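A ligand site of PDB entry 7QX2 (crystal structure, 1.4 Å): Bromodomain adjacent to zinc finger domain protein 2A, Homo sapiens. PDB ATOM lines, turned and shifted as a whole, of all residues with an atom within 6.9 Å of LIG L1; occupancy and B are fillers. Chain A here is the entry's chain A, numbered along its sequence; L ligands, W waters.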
ATOM      1  N   TRP A  23      11.663  -0.448 -11.856  1.00  0.00           N
ATOM      2  CA  TRP A  23      11.894  -0.926 -10.497  1.00  0.00           C
ATOM      3  C   TRP A  23      12.292  -2.399 -10.408  1.00  0.00           C
ATOM      4  O   TRP A  23      13.143  -2.719  -9.557  1.00  0.00           O
ATOM      5  CB  TRP A  23      10.691  -0.584  -9.599  1.00  0.00           C
ATOM      6  CG  TRP A  23       9.422  -1.206 -10.049  1.00  0.00           C
ATOM      7  CD1 TRP A  23       8.513  -0.670 -10.926  1.00  0.00           C
ATOM      8  CD2 TRP A  23       8.916  -2.490  -9.691  1.00  0.00           C
ATOM      9  NE1 TRP A  23       7.488  -1.553 -11.152  1.00  0.00           N
ATOM     10  CE2 TRP A  23       7.701  -2.678 -10.397  1.00  0.00           C
ATOM     11  CE3 TRP A  23       9.365  -3.522  -8.843  1.00  0.00           C
ATOM     12  CZ2 TRP A  23       6.938  -3.842 -10.289  1.00  0.00           C
ATOM     13  CZ3 TRP A  23       8.597  -4.678  -8.733  1.00  0.00           C
ATOM     14  CH2 TRP A  23       7.396  -4.821  -9.447  1.00  0.00           C
ATOM     15  N   PRO A  24      11.765  -3.319 -11.220  1.00  0.00           N
ATOM     16  CA  PRO A  24      12.217  -4.714 -11.074  1.00  0.00           C
ATOM     17  C   PRO A  24      13.664  -4.920 -11.430  1.00  0.00           C
ATOM     18  O   PRO A  24      14.225  -5.932 -10.996  1.00  0.00           O
ATOM     19  CB  PRO A  24      11.315  -5.493 -12.030  1.00  0.00           C
ATOM     20  CG  PRO A  24      10.154  -4.605 -12.277  1.00  0.00           C
ATOM     21  CD  PRO A  24      10.750  -3.227 -12.287  1.00  0.00           C
ATOM     22  N   PHE A  25      14.260  -4.027 -12.241  1.00  0.00           N
ATOM     23  CA  PHE A  25      15.496  -4.312 -12.955  1.00  0.00           C
ATOM     24  C   PHE A  25      16.686  -3.530 -12.422  1.00  0.00           C
ATOM     25  O   PHE A  25      17.768  -3.587 -13.011  1.00  0.00           O
ATOM     26  CB  PHE A  25      15.300  -4.035 -14.455  1.00  0.00           C
ATOM     27  CG  PHE A  25      14.049  -4.643 -14.988  1.00  0.00           C
ATOM     28  CD1 PHE A  25      13.915  -6.019 -15.040  1.00  0.00           C
ATOM     29  CD2 PHE A  25      12.961  -3.852 -15.379  1.00  0.00           C
ATOM     30  CE1 PHE A  25      12.761  -6.599 -15.491  1.00  0.00           C
ATOM     31  CE2 PHE A  25      11.791  -4.430 -15.826  1.00  0.00           C
ATOM     32  CZ  PHE A  25      11.685  -5.800 -15.884  1.00  0.00           C
ATOM     33  N   LEU A  26      16.519  -2.808 -11.312  1.00  0.00           N
ATOM     34  CA  LEU A  26      17.554  -1.901 -10.855  1.00  0.00           C
ATOM     35  C   LEU A  26      18.768  -2.640 -10.292  1.00  0.00           C
ATOM     36  O   LEU A  26      19.903  -2.175 -10.445  1.00  0.00           O
ATOM     37  CB  LEU A  26      16.990  -0.937  -9.814  1.00  0.00           C
ATOM     38  CG  LEU A  26      15.881  -0.028 -10.346  1.00  0.00           C
ATOM     39  CD1 LEU A  26      15.419   0.894  -9.205  1.00  0.00           C
ATOM     40  CD2 LEU A  26      16.287   0.789 -11.540  1.00  0.00           C
ATOM     41  N   GLU A  27      18.535  -3.776  -9.644  1.00  0.00           N
ATOM     42  CA  GLU A  27      19.558  -4.557  -8.986  1.00  0.00           C
ATOM     43  C   GLU A  27      19.407  -6.006  -9.408  1.00  0.00           C
ATOM     44  O   GLU A  27      18.364  -6.392  -9.951  1.00  0.00           O
ATOM     45  CB  GLU A  27      19.416  -4.438  -7.457  1.00  0.00           C
ATOM     46  CG  GLU A  27      19.634  -3.015  -6.935  1.00  0.00           C
ATOM     47  CD  GLU A  27      21.035  -2.508  -7.142  1.00  0.00           C
ATOM     48  OE1 GLU A  27      21.953  -3.350  -7.210  1.00  0.00           O
ATOM     49  OE2 GLU A  27      21.210  -1.265  -7.258  1.00  0.00           O
ATOM     50  N   PRO A  28      20.419  -6.834  -9.190  1.00  0.00           N
ATOM     51  CA  PRO A  28      20.289  -8.258  -9.551  1.00  0.00           C
ATOM     52  C   PRO A  28      19.035  -8.878  -8.954  1.00  0.00           C
ATOM     53  O   PRO A  28      18.608  -8.570  -7.832  1.00  0.00           O
ATOM     54  CB  PRO A  28      21.543  -8.880  -8.932  1.00  0.00           C
ATOM     55  CG  PRO A  28      22.538  -7.763  -8.883  1.00  0.00           C
ATOM     56  CD  PRO A  28      21.717  -6.523  -8.590  1.00  0.00           C
ATOM     57  N   VAL A  29      18.421  -9.812  -9.698  1.00  0.00           N
ATOM     58  CA  VAL A  29      17.301 -10.564  -9.115  1.00  0.00           C
ATOM     59  C   VAL A  29      17.748 -11.200  -7.811  1.00  0.00           C
ATOM     60  O   VAL A  29      18.787 -11.882  -7.744  1.00  0.00           O
ATOM     61  CB  VAL A  29      16.728 -11.592 -10.119  1.00  0.00           C
ATOM     62  CG1 VAL A  29      15.645 -12.453  -9.456  1.00  0.00           C
ATOM     63  CG2 VAL A  29      16.152 -10.868 -11.340  1.00  0.00           C
ATOM     64  N   ASN A  30      16.944 -11.004  -6.796  1.00  0.00           N
ATOM     65  CA  ASN A  30      17.347 -11.216  -5.409  1.00  0.00           C
ATOM     66  C   ASN A  30      16.865 -12.554  -4.863  1.00  0.00           C
ATOM     67  O   ASN A  30      15.651 -12.761  -4.716  1.00  0.00           O
ATOM     68  CB  ASN A  30      16.749 -10.068  -4.597  1.00  0.00           C
ATOM     69  CG  ASN A  30      17.345  -9.930  -3.203  1.00  0.00           C
ATOM     70  OD1 ASN A  30      17.886 -10.888  -2.617  1.00  0.00           O
ATOM     71  ND2 ASN A  30      17.180  -8.743  -2.626  1.00  0.00           N
ATOM     72  N   LEU A  33      14.116 -12.920  -2.340  1.00  0.00           N
ATOM     73  CA  LEU A  33      12.746 -12.648  -2.720  1.00  0.00           C
ATOM     74  C   LEU A  33      12.125 -13.695  -3.636  1.00  0.00           C
ATOM     75  O   LEU A  33      10.915 -13.670  -3.810  1.00  0.00           O
ATOM     76  CB  LEU A  33      12.662 -11.295  -3.441  1.00  0.00           C
ATOM     77  CG  LEU A  33      13.219 -10.111  -2.656  1.00  0.00           C
ATOM     78  CD1 LEU A  33      13.144  -8.829  -3.469  1.00  0.00           C
ATOM     79  CD2 LEU A  33      12.518  -9.923  -1.323  1.00  0.00           C
ATOM     80  N   VAL A  34      12.930 -14.548  -4.273  1.00  0.00           N
ATOM     81  CA  VAL A  34      12.397 -15.558  -5.184  1.00  0.00           C
ATOM     82  C   VAL A  34      13.431 -16.651  -5.297  1.00  0.00           C
ATOM     83  O   VAL A  34      14.642 -16.381  -5.353  1.00  0.00           O
ATOM     84  CB  VAL A  34      12.047 -14.937  -6.553  1.00  0.00           C
ATOM     85  CG1 VAL A  34      13.286 -14.325  -7.212  1.00  0.00           C
ATOM     86  CG2 VAL A  34      11.379 -15.980  -7.443  1.00  0.00           C
ATOM     87  N   TYR A  37      15.698 -18.838  -9.498  1.00  0.00           N
ATOM     88  CA  TYR A  37      15.929 -17.925 -10.606  1.00  0.00           C
ATOM     89  C   TYR A  37      17.157 -18.337 -11.413  1.00  0.00           C
ATOM     90  O   TYR A  37      17.043 -18.624 -12.605  1.00  0.00           O
ATOM     91  CB  TYR A  37      16.024 -16.473 -10.114  1.00  0.00           C
ATOM     92  CG  TYR A  37      16.091 -15.506 -11.264  1.00  0.00           C
ATOM     93  CD1 TYR A  37      14.945 -15.139 -11.934  1.00  0.00           C
ATOM     94  CD2 TYR A  37      17.310 -14.990 -11.707  1.00  0.00           C
ATOM     95  CE1 TYR A  37      14.986 -14.258 -13.003  1.00  0.00           C
ATOM     96  CE2 TYR A  37      17.371 -14.111 -12.767  1.00  0.00           C
ATOM     97  CZ  TYR A  37      16.213 -13.764 -13.427  1.00  0.00           C
ATOM     98  OH  TYR A  37      16.300 -12.892 -14.500  1.00  0.00           O
ATOM     99  N   MET A  45      21.051 -10.395 -15.556  1.00  0.00           N
ATOM    100  CA  MET A  45      21.504  -9.054 -15.877  1.00  0.00           C
ATOM    101  C   MET A  45      20.550  -8.038 -15.257  1.00  0.00           C
ATOM    102  O   MET A  45      19.374  -8.324 -15.064  1.00  0.00           O
ATOM    103  CB  MET A  45      21.676  -8.844 -17.402  1.00  0.00           C
ATOM    104  CG  MET A  45      22.331  -7.517 -17.854  1.00  0.00           C
ATOM    105  SD  MET A  45      23.879  -7.158 -17.000  1.00  0.00           S
ATOM    106  CE  MET A  45      24.792  -8.663 -17.334  1.00  0.00           C
ATOM    107  N   VAL A  72      18.382  -8.236 -20.046  1.00  0.00           N
ATOM    108  CA  VAL A  72      17.468  -7.942 -18.944  1.00  0.00           C
ATOM    109  C   VAL A  72      16.040  -8.317 -19.325  1.00  0.00           C
ATOM    110  O   VAL A  72      15.320  -8.970 -18.555  1.00  0.00           O
ATOM    111  CB  VAL A  72      17.541  -6.452 -18.547  1.00  0.00           C
ATOM    112  CG1 VAL A  72      16.496  -6.149 -17.453  1.00  0.00           C
ATOM    113  CG2 VAL A  72      18.934  -6.070 -18.057  1.00  0.00           C
ATOM    114  N   ASN A  75      15.554 -12.203 -20.147  1.00  0.00           N
ATOM    115  CA  ASN A  75      15.439 -12.979 -18.918  1.00  0.00           C
ATOM    116  C   ASN A  75      14.076 -12.773 -18.290  1.00  0.00           C
ATOM    117  O   ASN A  75      13.455 -13.726 -17.810  1.00  0.00           O
ATOM    118  CB  ASN A  75      16.528 -12.563 -17.934  1.00  0.00           C
ATOM    119  CG  ASN A  75      17.907 -12.982 -18.346  1.00  0.00           C
ATOM    120  OD1 ASN A  75      18.095 -13.867 -19.186  1.00  0.00           O
ATOM    121  ND2 ASN A  75      18.895 -12.376 -17.713  1.00  0.00           N
ATOM    122  N   CYS A  76      13.604 -11.527 -18.245  1.00  0.00           N
ATOM    123  CA  CYS A  76      12.300 -11.223 -17.660  1.00  0.00           C
ATOM    124  C   CYS A  76      11.198 -12.038 -18.323  1.00  0.00           C
ATOM    125  O   CYS A  76      10.350 -12.631 -17.644  1.00  0.00           O
ATOM    126  CB  CYS A  76      12.021  -9.727 -17.759  1.00  0.00           C
ATOM    127  SG  CYS A  76      10.531  -9.200 -16.920  1.00  0.00           S
ATOM    128  N   PHE A  79      11.341 -15.842 -17.384  1.00  0.00           N
ATOM    129  CA  PHE A  79      11.035 -16.271 -16.031  1.00  0.00           C
ATOM    130  C   PHE A  79       9.633 -15.916 -15.589  1.00  0.00           C
ATOM    131  O   PHE A  79       9.057 -16.646 -14.774  1.00  0.00           O
ATOM    132  CB  PHE A  79      12.014 -15.627 -15.047  1.00  0.00           C
ATOM    133  CG  PHE A  79      11.995 -16.277 -13.702  1.00  0.00           C
ATOM    134  CD1 PHE A  79      12.640 -17.478 -13.514  1.00  0.00           C
ATOM    135  CD2 PHE A  79      11.297 -15.727 -12.640  1.00  0.00           C
ATOM    136  CE1 PHE A  79      12.640 -18.104 -12.309  1.00  0.00           C
ATOM    137  CE2 PHE A  79      11.290 -16.349 -11.412  1.00  0.00           C
ATOM    138  CZ  PHE A  79      11.954 -17.548 -11.249  1.00  0.00           C
ATOM    139  N   ASN A  80       9.102 -14.791 -16.038  1.00  0.00           N
ATOM    140  CA  ASN A  80       7.867 -14.229 -15.512  1.00  0.00           C
ATOM    141  C   ASN A  80       6.762 -14.355 -16.550  1.00  0.00           C
ATOM    142  O   ASN A  80       7.015 -14.295 -17.752  1.00  0.00           O
ATOM    143  CB  ASN A  80       8.059 -12.745 -15.162  1.00  0.00           C
ATOM    144  CG  ASN A  80       9.154 -12.527 -14.147  1.00  0.00           C
ATOM    145  OD1 ASN A  80       8.951 -12.699 -12.946  1.00  0.00           O
ATOM    146  ND2 ASN A  80      10.332 -12.146 -14.617  1.00  0.00           N
ATOM    147  N   VAL A  86       5.984  -7.775 -12.823  1.00  0.00           N
ATOM    148  CA  VAL A  86       7.327  -7.739 -13.369  1.00  0.00           C
ATOM    149  C   VAL A  86       7.301  -8.015 -14.869  1.00  0.00           C
ATOM    150  O   VAL A  86       8.016  -7.386 -15.655  1.00  0.00           O
ATOM    151  CB  VAL A  86       8.244  -8.715 -12.603  1.00  0.00           C
ATOM    152  CG1 VAL A  86       9.585  -8.810 -13.265  1.00  0.00           C
ATOM    153  CG2 VAL A  86       8.412  -8.252 -11.181  1.00  0.00           C
HETATM  154  C1  LIG L   1      11.444 -11.219  -7.144  1.00  0.00           C
HETATM  155  C2  LIG L   1      10.682 -10.715  -8.366  1.00  0.00           C
HETATM  156  C3  LIG L   1      11.537  -9.872  -9.329  1.00  0.00           C
HETATM  157  C4  LIG L   1      11.854  -8.564  -9.095  1.00  0.00           C
HETATM  158  C5  LIG L   1      12.707  -9.046 -11.048  1.00  0.00           C
HETATM  159  C6  LIG L   1      13.443  -8.836 -12.353  1.00  0.00           C
HETATM  160  C7  LIG L   1      12.059 -10.172 -10.594  1.00  0.00           C
HETATM  161  C8  LIG L   1      12.044 -11.483 -11.371  1.00  0.00           C
HETATM  162  C9  LIG L   1      11.714 -12.807 -10.683  1.00  0.00           C
HETATM  163  C10 LIG L   1      11.567  -7.676  -7.922  1.00  0.00           C
HETATM  164  C11 LIG L   1      10.625  -7.809  -6.859  1.00  0.00           C
HETATM  165  C12 LIG L   1      11.933  -5.755  -6.659  1.00  0.00           C
HETATM  166  C13 LIG L   1      12.563  -4.448  -6.209  1.00  0.00           C
HETATM  167  C14 LIG L   1      12.656  -3.146  -4.393  1.00  0.00           C
HETATM  168  C15 LIG L   1      12.770  -3.162  -2.861  1.00  0.00           C
HETATM  169  C16 LIG L   1      13.906  -3.920  -2.377  1.00  0.00           C
HETATM  170  C17 LIG L   1      13.996  -5.221  -3.002  1.00  0.00           C
HETATM  171  C18 LIG L   1      13.810  -5.203  -4.511  1.00  0.00           C
HETATM  172  N1  LIG L   1      12.573  -8.099 -10.122  1.00  0.00           N
HETATM  173  N2  LIG L   1      12.645  -4.468  -4.961  1.00  0.00           N
HETATM  174  N3  LIG L   1      13.843  -4.081  -0.917  1.00  0.00           N
HETATM  175  N4  LIG L   1      12.325  -6.453  -7.779  1.00  0.00           N
HETATM  176  O1  LIG L   1      12.350 -11.483 -12.522  1.00  0.00           O
HETATM  177  S1  LIG L   1      10.738  -6.552  -5.852  1.00  0.00           S
HETATM  178  C1  LG2 L   2       8.818  -2.964  -4.467  1.00  0.00           C
HETATM  179  C2  LG2 L   2       7.854  -3.598  -3.462  1.00  0.00           C
HETATM  180  C3  LG2 L   2       7.855  -5.116  -3.595  1.00  0.00           C
HETATM  181  C4  LG2 L   2       7.060  -5.852  -4.456  1.00  0.00           C
HETATM  182  C5  LG2 L   2       8.298  -7.279  -3.393  1.00  0.00           C
HETATM  183  C6  LG2 L   2       8.886  -8.602  -2.959  1.00  0.00           C
HETATM  184  C7  LG2 L   2       8.653  -6.036  -2.931  1.00  0.00           C
HETATM  185  C8  LG2 L   2       9.694  -5.840  -1.833  1.00  0.00           C
HETATM  186  C9  LG2 L   2       9.540  -4.697  -0.833  1.00  0.00           C
HETATM  187  C10 LG2 L   2       5.982  -5.388  -5.402  1.00  0.00           C
HETATM  188  C11 LG2 L   2       5.479  -6.116  -6.507  1.00  0.00           C
HETATM  189  C12 LG2 L   2       4.233  -4.007  -6.178  1.00  0.00           C
HETATM  190  C13 LG2 L   2       3.310  -2.795  -6.256  1.00  0.00           C
HETATM  191  C14 LG2 L   2       2.670  -2.265  -8.372  1.00  0.00           C
HETATM  192  C15 LG2 L   2       2.868  -1.262  -9.504  1.00  0.00           C
HETATM  193  C16 LG2 L   2       4.229  -0.833  -9.722  1.00  0.00           C
HETATM  194  C17 LG2 L   2       4.965  -0.513  -8.522  1.00  0.00           C
HETATM  195  C18 LG2 L   2       4.865  -1.581  -7.429  1.00  0.00           C
HETATM  196  N1  LG2 L   2       7.351  -7.153  -4.306  1.00  0.00           N
HETATM  197  N2  LG2 L   2       3.518  -2.069  -7.232  1.00  0.00           N
HETATM  198  N3  LG2 L   2       4.214   0.350 -10.575  1.00  0.00           N
HETATM  199  N4  LG2 L   2       5.205  -4.154  -5.199  1.00  0.00           N
HETATM  200  O1  LG2 L   2      10.560  -6.623  -1.676  1.00  0.00           O
HETATM  201  S1  LG2 L   2       4.263  -5.298  -7.195  1.00  0.00           S
HETATM  202  O   HOH W   1      13.688  -1.407  -7.141  1.00  0.00           O
HETATM  203  O   HOH W   2      12.262  -5.917   0.286  1.00  0.00           O
HETATM  204  O   HOH W   3      14.668  -9.192  -7.146  1.00  0.00           O
HETATM  205  O   HOH W   4      14.053 -11.493 -14.849  1.00  0.00           O
HETATM  206  O   HOH W   5      16.460  -7.513 -11.443  1.00  0.00           O
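ND2 of Asn 80 sits at hydrogen-bond distance from O of Cys 76 (3.1 Å). O of Val 86 lies within hydrogen-bond range of SG of Cys 76 (3.3 Å).
A nitrogen (N1) of LG2 L2 lies close to a sulfur (S1) of LIG L1 (3.8 Å).
Trp 23 touches LIG L1 (O to C13, 3.8 Å). Phe 25 touches LIG L1. Val 29 touches LIG L1 (CG2 to C6, 3.5 Å). Leu 33 touches LIG L1 (CD1 to C17, 3.7 Å). Val 34 touches LIG L1 (CG1 to C1, 3.6 Å). CE1 of Tyr 37 touches O1 of LIG L1, 3.9 Å away. Phe 79 touches LIG L1. Val 86 touches LIG L1 (CG1 to C5, 3.8 Å). Hydrophobic or aromatic side chains that line LIG L1: Pro 24, Phe 25, Val 29, Leu 33, Val 34, Tyr 37, Phe 79 and Val 86. Ten residues have an atom within 4 Å of LIG L1: Trp 23, Pro 24, Phe 25, Val 29, Leu 33, Val 34, Tyr 37, Phe 79, Asn 80 and Val 86. The nearest printed residue that does not touch LIG L1 is Asn 30 (4.8 Å).
The backbone carbonyl oxygen (O) of Pro 24 is in hydrogen-bond range of a nitrogen (N1) of LIG L1, 2.9 Å away. The side-chain amide nitrogen of Asn 80 sits at hydrogen-bond distance from an oxygen (O1) of LIG L1, at 3.0 Å.
Water W2 bridges O1 of LG2 L2 and N3 of LIG L1. Water W4 lies within hydrogen-bond range of the side-chain hydroxyl (OH) of Tyr 37 (2.7 Å), an oxygen (O1) of LIG L1 (2.9 Å) and the backbone NH (N) of Cys 76 (3.4 Å). Water W5 lies within hydrogen-bond range of the backbone carbonyl oxygen of Glu 27, the backbone carbonyl oxygen of Pro 24 and the backbone NH of Val 29.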
